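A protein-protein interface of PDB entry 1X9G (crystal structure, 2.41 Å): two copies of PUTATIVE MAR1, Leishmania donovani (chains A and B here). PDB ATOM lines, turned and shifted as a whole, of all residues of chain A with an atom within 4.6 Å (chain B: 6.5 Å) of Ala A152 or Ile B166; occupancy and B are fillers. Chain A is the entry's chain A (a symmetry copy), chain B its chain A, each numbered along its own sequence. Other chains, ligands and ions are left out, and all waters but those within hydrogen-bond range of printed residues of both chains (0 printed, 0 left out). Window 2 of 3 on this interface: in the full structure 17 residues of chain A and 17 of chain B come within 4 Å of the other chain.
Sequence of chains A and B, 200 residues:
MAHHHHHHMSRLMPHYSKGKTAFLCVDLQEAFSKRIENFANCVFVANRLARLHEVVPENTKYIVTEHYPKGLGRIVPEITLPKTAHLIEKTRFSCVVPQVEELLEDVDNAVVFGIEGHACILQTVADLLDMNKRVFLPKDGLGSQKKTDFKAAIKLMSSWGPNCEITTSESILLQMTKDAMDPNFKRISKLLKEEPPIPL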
ATOM      1  N   THR A 148       7.024 -24.969 -20.951  1.00  0.00           N
ATOM      2  CA  THR A 148       7.177 -23.847 -21.873  1.00  0.00           C
ATOM      3  C   THR A 148       6.032 -22.856 -21.718  1.00  0.00           C
ATOM      4  O   THR A 148       6.239 -21.657 -21.689  1.00  0.00           O
ATOM      5  CB  THR A 148       7.374 -24.333 -23.349  1.00  0.00           C
ATOM      6  OG1 THR A 148       8.502 -25.205 -23.420  1.00  0.00           O
ATOM      7  CG2 THR A 148       7.630 -23.180 -24.323  1.00  0.00           C
ATOM      8  N   ASP A 149       4.825 -23.362 -21.586  1.00  0.00           N
ATOM      9  CA  ASP A 149       3.670 -22.517 -21.368  1.00  0.00           C
ATOM     10  C   ASP A 149       3.762 -21.817 -20.012  1.00  0.00           C
ATOM     11  O   ASP A 149       3.471 -20.644 -19.906  1.00  0.00           O
ATOM     12  CB  ASP A 149       2.372 -23.337 -21.446  1.00  0.00           C
ATOM     13  CG  ASP A 149       2.117 -23.979 -22.845  1.00  0.00           C
ATOM     14  OD1 ASP A 149       2.122 -23.281 -23.858  1.00  0.00           O
ATOM     15  OD2 ASP A 149       1.844 -25.185 -22.908  1.00  0.00           O
ATOM     16  N   PHE A 150       4.153 -22.552 -18.983  1.00  0.00           N
ATOM     17  CA  PHE A 150       4.238 -22.016 -17.609  1.00  0.00           C
ATOM     18  C   PHE A 150       5.270 -20.928 -17.540  1.00  0.00           C
ATOM     19  O   PHE A 150       4.948 -19.775 -17.223  1.00  0.00           O
ATOM     20  CB  PHE A 150       4.596 -23.138 -16.628  1.00  0.00           C
ATOM     21  CG  PHE A 150       4.530 -22.737 -15.207  1.00  0.00           C
ATOM     22  CD1 PHE A 150       5.713 -22.483 -14.474  1.00  0.00           C
ATOM     23  CD2 PHE A 150       3.315 -22.628 -14.573  1.00  0.00           C
ATOM     24  CE1 PHE A 150       5.673 -22.112 -13.158  1.00  0.00           C
ATOM     25  CE2 PHE A 150       3.264 -22.264 -13.236  1.00  0.00           C
ATOM     26  CZ  PHE A 150       4.449 -21.991 -12.527  1.00  0.00           C
ATOM     27  N   LYS A 151       6.503 -21.299 -17.893  1.00  0.00           N
ATOM     28  CA  LYS A 151       7.669 -20.441 -17.776  1.00  0.00           C
ATOM     29  C   LYS A 151       7.472 -19.098 -18.476  1.00  0.00           C
ATOM     30  O   LYS A 151       7.888 -18.074 -17.965  1.00  0.00           O
ATOM     31  CB  LYS A 151       8.921 -21.165 -18.309  1.00  0.00           C
ATOM     32  CG  LYS A 151       9.478 -22.238 -17.335  1.00  0.00           C
ATOM     33  CD  LYS A 151      10.927 -22.722 -17.638  1.00  0.00           C
ATOM     34  CE  LYS A 151      11.982 -21.557 -17.372  1.00  0.00           C
ATOM     35  NZ  LYS A 151      13.410 -21.748 -17.964  1.00  0.00           N
ATOM     36  N   ALA A 152       6.821 -19.110 -19.634  1.00  0.00           N
ATOM     37  CA  ALA A 152       6.493 -17.906 -20.410  1.00  0.00           C
ATOM     38  C   ALA A 152       5.417 -17.030 -19.741  1.00  0.00           C
ATOM     39  O   ALA A 152       5.573 -15.816 -19.612  1.00  0.00           O
ATOM     40  CB  ALA A 152       6.070 -18.313 -21.845  1.00  0.00           C
ATOM     41  N   ALA A 153       4.330 -17.635 -19.268  1.00  0.00           N
ATOM     42  CA  ALA A 153       3.278 -16.873 -18.573  1.00  0.00           C
ATOM     43  C   ALA A 153       3.859 -16.221 -17.302  1.00  0.00           C
ATOM     44  O   ALA A 153       3.603 -15.041 -17.016  1.00  0.00           O
ATOM     45  CB  ALA A 153       2.114 -17.786 -18.249  1.00  0.00           C
ATOM     46  N   ILE A 154       4.668 -16.977 -16.558  1.00  0.00           N
ATOM     47  CA  ILE A 154       5.402 -16.440 -15.341  1.00  0.00           C
ATOM     48  C   ILE A 154       6.274 -15.207 -15.597  1.00  0.00           C
ATOM     49  O   ILE A 154       6.134 -14.233 -14.856  1.00  0.00           O
ATOM     50  CB  ILE A 154       6.275 -17.510 -14.639  1.00  0.00           C
ATOM     51  CG1 ILE A 154       5.415 -18.599 -14.067  1.00  0.00           C
ATOM     52  CG2 ILE A 154       7.060 -16.889 -13.490  1.00  0.00           C
ATOM     53  CD1 ILE A 154       4.412 -18.046 -13.158  1.00  0.00           C
ATOM     54  N   LYS A 155       7.129 -15.248 -16.630  1.00  0.00           N
ATOM     55  CA  LYS A 155       7.867 -14.048 -17.053  1.00  0.00           C
ATOM     56  C   LYS A 155       6.968 -12.917 -17.482  1.00  0.00           C
ATOM     57  O   LYS A 155       7.195 -11.808 -17.113  1.00  0.00           O
ATOM     58  CB  LYS A 155       8.836 -14.236 -18.250  1.00  0.00           C
ATOM     59  CG  LYS A 155       9.639 -15.472 -18.381  1.00  0.00           C
ATOM     60  CD  LYS A 155      10.788 -15.563 -17.391  1.00  0.00           C
ATOM     61  CE  LYS A 155      12.018 -16.248 -18.084  1.00  0.00           C
ATOM     62  NZ  LYS A 155      13.210 -16.207 -17.182  1.00  0.00           N
ATOM     63  N   LEU A 156       5.963 -13.158 -18.296  1.00  0.00           N
ATOM     64  CA  LEU A 156       5.075 -12.057 -18.660  1.00  0.00           C
ATOM     65  C   LEU A 156       4.607 -11.361 -17.358  1.00  0.00           C
ATOM     66  O   LEU A 156       4.716 -10.151 -17.205  1.00  0.00           O
ATOM     67  CB  LEU A 156       3.818 -12.597 -19.351  1.00  0.00           C
ATOM     68  CG  LEU A 156       3.318 -11.810 -20.549  1.00  0.00           C
ATOM     69  CD1 LEU A 156       1.796 -11.987 -20.734  1.00  0.00           C
ATOM     70  CD2 LEU A 156       3.788 -10.316 -20.589  1.00  0.00           C
ATOM     71  N   VAL B 135       2.091  -6.259 -30.191  1.00  0.00           N
ATOM     72  CA  VAL B 135       2.650  -7.501 -30.665  1.00  0.00           C
ATOM     73  C   VAL B 135       2.671  -8.664 -29.657  1.00  0.00           C
ATOM     74  O   VAL B 135       2.938  -8.472 -28.468  1.00  0.00           O
ATOM     75  CB  VAL B 135       3.910  -7.316 -31.620  1.00  0.00           C
ATOM     76  CG1 VAL B 135       4.334  -5.895 -31.779  1.00  0.00           C
ATOM     77  CG2 VAL B 135       5.026  -8.269 -31.308  1.00  0.00           C
ATOM     78  N   PHE B 136       2.301  -9.849 -30.149  1.00  0.00           N
ATOM     79  CA  PHE B 136       2.150 -11.065 -29.355  1.00  0.00           C
ATOM     80  C   PHE B 136       2.887 -12.171 -30.018  1.00  0.00           C
ATOM     81  O   PHE B 136       2.758 -12.362 -31.230  1.00  0.00           O
ATOM     82  CB  PHE B 136       0.681 -11.461 -29.220  1.00  0.00           C
ATOM     83  CG  PHE B 136      -0.174 -10.369 -28.680  1.00  0.00           C
ATOM     84  CD1 PHE B 136      -0.699  -9.400 -29.539  1.00  0.00           C
ATOM     85  CD2 PHE B 136      -0.439 -10.287 -27.304  1.00  0.00           C
ATOM     86  CE1 PHE B 136      -1.499  -8.364 -29.020  1.00  0.00           C
ATOM     87  CE2 PHE B 136      -1.202  -9.264 -26.772  1.00  0.00           C
ATOM     88  CZ  PHE B 136      -1.753  -8.308 -27.636  1.00  0.00           C
ATOM     89  N   LEU B 137       3.676 -12.905 -29.239  1.00  0.00           N
ATOM     90  CA  LEU B 137       4.650 -13.801 -29.826  1.00  0.00           C
ATOM     91  C   LEU B 137       4.546 -15.143 -29.141  1.00  0.00           C
ATOM     92  O   LEU B 137       4.703 -15.225 -27.958  1.00  0.00           O
ATOM     93  CB  LEU B 137       6.080 -13.197 -29.667  1.00  0.00           C
ATOM     94  CG  LEU B 137       6.352 -11.865 -30.388  1.00  0.00           C
ATOM     95  CD1 LEU B 137       6.954 -10.883 -29.488  1.00  0.00           C
ATOM     96  CD2 LEU B 137       7.250 -12.093 -31.616  1.00  0.00           C
ATOM     97  N   PRO B 138       4.239 -16.211 -29.891  1.00  0.00           N
ATOM     98  CA  PRO B 138       4.298 -17.511 -29.239  1.00  0.00           C
ATOM     99  C   PRO B 138       5.724 -18.019 -29.265  1.00  0.00           C
ATOM    100  O   PRO B 138       6.207 -18.361 -30.359  1.00  0.00           O
ATOM    101  CB  PRO B 138       3.432 -18.382 -30.146  1.00  0.00           C
ATOM    102  CG  PRO B 138       3.673 -17.790 -31.540  1.00  0.00           C
ATOM    103  CD  PRO B 138       3.803 -16.306 -31.307  1.00  0.00           C
ATOM    104  N   LYS B 139       6.380 -18.073 -28.101  1.00  0.00           N
ATOM    105  CA  LYS B 139       7.774 -18.545 -27.983  1.00  0.00           C
ATOM    106  C   LYS B 139       7.965 -19.945 -28.530  1.00  0.00           C
ATOM    107  O   LYS B 139       9.050 -20.342 -28.970  1.00  0.00           O
ATOM    108  CB  LYS B 139       8.224 -18.535 -26.527  1.00  0.00           C
ATOM    109  CG  LYS B 139       9.724 -18.773 -26.389  1.00  0.00           C
ATOM    110  CD  LYS B 139      10.155 -18.612 -24.932  1.00  0.00           C
ATOM    111  CE  LYS B 139      11.255 -19.560 -24.581  1.00  0.00           C
ATOM    112  NZ  LYS B 139      12.130 -18.844 -23.593  1.00  0.00           N
ATOM    113  N   LEU B 142       8.984 -19.808 -32.231  1.00  0.00           N
ATOM    114  CA  LEU B 142      10.205 -19.059 -32.557  1.00  0.00           C
ATOM    115  C   LEU B 142      11.444 -19.950 -32.457  1.00  0.00           C
ATOM    116  O   LEU B 142      11.439 -20.978 -31.746  1.00  0.00           O
ATOM    117  CB  LEU B 142      10.377 -17.808 -31.694  1.00  0.00           C
ATOM    118  CG  LEU B 142       9.276 -16.753 -31.520  1.00  0.00           C
ATOM    119  CD1 LEU B 142       9.521 -15.926 -30.230  1.00  0.00           C
ATOM    120  CD2 LEU B 142       9.021 -15.859 -32.768  1.00  0.00           C
ATOM    121  N   ALA B 153      17.899 -12.277 -27.691  1.00  0.00           N
ATOM    122  CA  ALA B 153      16.842 -11.528 -28.392  1.00  0.00           C
ATOM    123  C   ALA B 153      15.516 -11.642 -27.614  1.00  0.00           C
ATOM    124  O   ALA B 153      14.801 -10.647 -27.422  1.00  0.00           O
ATOM    125  CB  ALA B 153      16.704 -12.045 -29.810  1.00  0.00           C
ATOM    126  N   ILE B 154      15.205 -12.848 -27.136  1.00  0.00           N
ATOM    127  CA  ILE B 154      13.991 -13.093 -26.257  1.00  0.00           C
ATOM    128  C   ILE B 154      13.913 -12.228 -24.996  1.00  0.00           C
ATOM    129  O   ILE B 154      12.865 -11.621 -24.771  1.00  0.00           O
ATOM    130  CB  ILE B 154      13.838 -14.575 -25.833  1.00  0.00           C
ATOM    131  CG1 ILE B 154      13.573 -15.441 -27.031  1.00  0.00           C
ATOM    132  CG2 ILE B 154      12.663 -14.739 -24.876  1.00  0.00           C
ATOM    133  CD1 ILE B 154      12.399 -14.969 -27.764  1.00  0.00           C
ATOM    134  N   LYS B 155      15.002 -12.161 -24.214  1.00  0.00           N
ATOM    135  CA  LYS B 155      15.073 -11.216 -23.090  1.00  0.00           C
ATOM    136  C   LYS B 155      14.948  -9.774 -23.515  1.00  0.00           C
ATOM    137  O   LYS B 155      14.248  -9.035 -22.900  1.00  0.00           O
ATOM    138  CB  LYS B 155      16.381 -11.251 -22.255  1.00  0.00           C
ATOM    139  CG  LYS B 155      17.049 -12.538 -21.959  1.00  0.00           C
ATOM    140  CD  LYS B 155      16.322 -13.379 -20.922  1.00  0.00           C
ATOM    141  CE  LYS B 155      17.374 -14.122 -20.026  1.00  0.00           C
ATOM    142  NZ  LYS B 155      16.690 -14.830 -18.901  1.00  0.00           N
ATOM    143  N   MET B 157      13.334  -8.494 -25.975  1.00  0.00           N
ATOM    144  CA  MET B 157      11.936  -8.268 -26.327  1.00  0.00           C
ATOM    145  C   MET B 157      10.967  -8.323 -25.114  1.00  0.00           C
ATOM    146  O   MET B 157      10.012  -7.579 -25.101  1.00  0.00           O
ATOM    147  CB  MET B 157      11.456  -9.253 -27.407  1.00  0.00           C
ATOM    148  CG  MET B 157      12.103  -9.034 -28.783  1.00  0.00           C
ATOM    149  SD  MET B 157      11.438 -10.051 -30.140  1.00  0.00           S
ATOM    150  CE  MET B 157      12.215 -11.654 -29.867  1.00  0.00           C
ATOM    151  N   SER B 158      11.212  -9.199 -24.133  1.00  0.00           N
ATOM    152  CA  SER B 158      10.474  -9.238 -22.859  1.00  0.00           C
ATOM    153  C   SER B 158      10.495  -7.901 -22.082  1.00  0.00           C
ATOM    154  O   SER B 158       9.682  -7.667 -21.189  1.00  0.00           O
ATOM    155  CB  SER B 158      11.103 -10.310 -21.950  1.00  0.00           C
ATOM    156  OG  SER B 158      10.600 -11.603 -22.276  1.00  0.00           O
ATOM    157  N   CYS B 164       4.357  -5.312 -26.151  1.00  0.00           N
ATOM    158  CA  CYS B 164       4.916  -6.564 -26.646  1.00  0.00           C
ATOM    159  C   CYS B 164       4.745  -7.668 -25.601  1.00  0.00           C
ATOM    160  O   CYS B 164       5.006  -7.455 -24.448  1.00  0.00           O
ATOM    161  CB  CYS B 164       6.389  -6.366 -26.995  1.00  0.00           C
ATOM    162  SG  CYS B 164       7.142  -7.754 -27.795  1.00  0.00           S
ATOM    163  N   GLU B 165       4.267  -8.847 -25.997  1.00  0.00           N
ATOM    164  CA  GLU B 165       4.067  -9.940 -25.027  1.00  0.00           C
ATOM    165  C   GLU B 165       4.435 -11.278 -25.556  1.00  0.00           C
ATOM    166  O   GLU B 165       3.951 -11.669 -26.618  1.00  0.00           O
ATOM    167  CB  GLU B 165       2.627 -10.023 -24.535  1.00  0.00           C
ATOM    168  CG  GLU B 165       2.049  -8.700 -24.022  1.00  0.00           C
ATOM    169  CD  GLU B 165       0.622  -8.866 -23.451  1.00  0.00           C
ATOM    170  OE1 GLU B 165       0.133  -7.877 -22.876  1.00  0.00           O
ATOM    171  OE2 GLU B 165       0.002  -9.961 -23.605  1.00  0.00           O
ATOM    172  N   ILE B 166       5.274 -11.986 -24.815  1.00  0.00           N
ATOM    173  CA  ILE B 166       5.728 -13.299 -25.210  1.00  0.00           C
ATOM    174  C   ILE B 166       5.008 -14.319 -24.365  1.00  0.00           C
ATOM    175  O   ILE B 166       5.122 -14.314 -23.130  1.00  0.00           O
ATOM    176  CB  ILE B 166       7.280 -13.437 -25.093  1.00  0.00           C
ATOM    177  CG1 ILE B 166       7.962 -12.386 -25.981  1.00  0.00           C
ATOM    178  CG2 ILE B 166       7.790 -14.844 -25.545  1.00  0.00           C
ATOM    179  CD1 ILE B 166       9.399 -12.315 -25.743  1.00  0.00           C
ATOM    180  N   THR B 167       4.227 -15.176 -25.011  1.00  0.00           N
ATOM    181  CA  THR B 167       3.587 -16.281 -24.278  1.00  0.00           C
ATOM    182  C   THR B 167       3.819 -17.537 -25.117  1.00  0.00           C
ATOM    183  O   THR B 167       4.950 -17.835 -25.468  1.00  0.00           O
ATOM    184  CB  THR B 167       2.076 -16.027 -23.974  1.00  0.00           C
ATOM    185  OG1 THR B 167       1.429 -15.527 -25.165  1.00  0.00           O
ATOM    186  CG2 THR B 167       1.868 -15.008 -22.789  1.00  0.00           C
ATOM    187  N   THR B 168       2.745 -18.246 -25.458  1.00  0.00           N
ATOM    188  CA  THR B 168       2.814 -19.420 -26.293  1.00  0.00           C
ATOM    189  C   THR B 168       1.530 -19.474 -27.054  1.00  0.00           C
ATOM    190  O   THR B 168       0.592 -18.746 -26.747  1.00  0.00           O
ATOM    191  CB  THR B 168       3.007 -20.760 -25.495  1.00  0.00           C
ATOM    192  OG1 THR B 168       1.998 -20.880 -24.492  1.00  0.00           O
ATOM    193  CG2 THR B 168       4.364 -20.844 -24.812  1.00  0.00           C
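Thr A148 touches Thr B168 (O to CG2, 3.7 Å). Ala A152 touches Ile B166 (O to O, 3.9 Å). O of Thr B167 touches CB of Ala A152, at 3.8 Å. Leu A156 touches Glu B165 (CD1 to OE2, 3.9 Å). Thr B167 touches Leu A156.
Positions printed for both chains: 153, 154 and 155.
Printed residues of chain B that touch a printed residue of chain A: Glu B165, Ile B166, Thr B167 and Thr B168. Hydrophobic or aromatic side chains of chain A that line the printed part of chain B: Ala A152 and Leu A156. Among the printed residues, 6 pairs touch across the chains. Among the printed residues, no Asp or Glu carboxylate lies within 4 Å of a Lys or Arg side-chain nitrogen of the other chain.
Ala A152 touches two residues of chain B. Printed residues of chain A within 4 Å of Glu B165: Leu A156. Of chain A, only Ala A152 comes within 4 Å of Ile B166. Of the printed residues of chain A, Thr B168 touches Thr A148 and Asp A149. The nearest residue of chain B that does not touch Ala A152 is Thr B168 (4.3 Å).
The side-chain hydroxyl (OG1) of Thr B168 sits at hydrogen-bond distance from the side-chain carboxylate (OD1) of Asp A149 (2.5 Å).
The backbone carbonyl oxygen (O) of Val B135 is in hydrogen-bond range of the backbone NH (N) of Glu B165, 2.8 Å away. The backbone NH of Leu B137 sits at hydrogen-bond distance from the backbone carbonyl oxygen of Glu B165 (2.9 Å). The backbone carbonyl oxygen (O) of Leu B137 lies within hydrogen-bond range of the backbone NH (N) of Thr B167 (3.0 Å). N of Lys B139 is in hydrogen-bond range of O of Thr B167 (3.0 Å).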
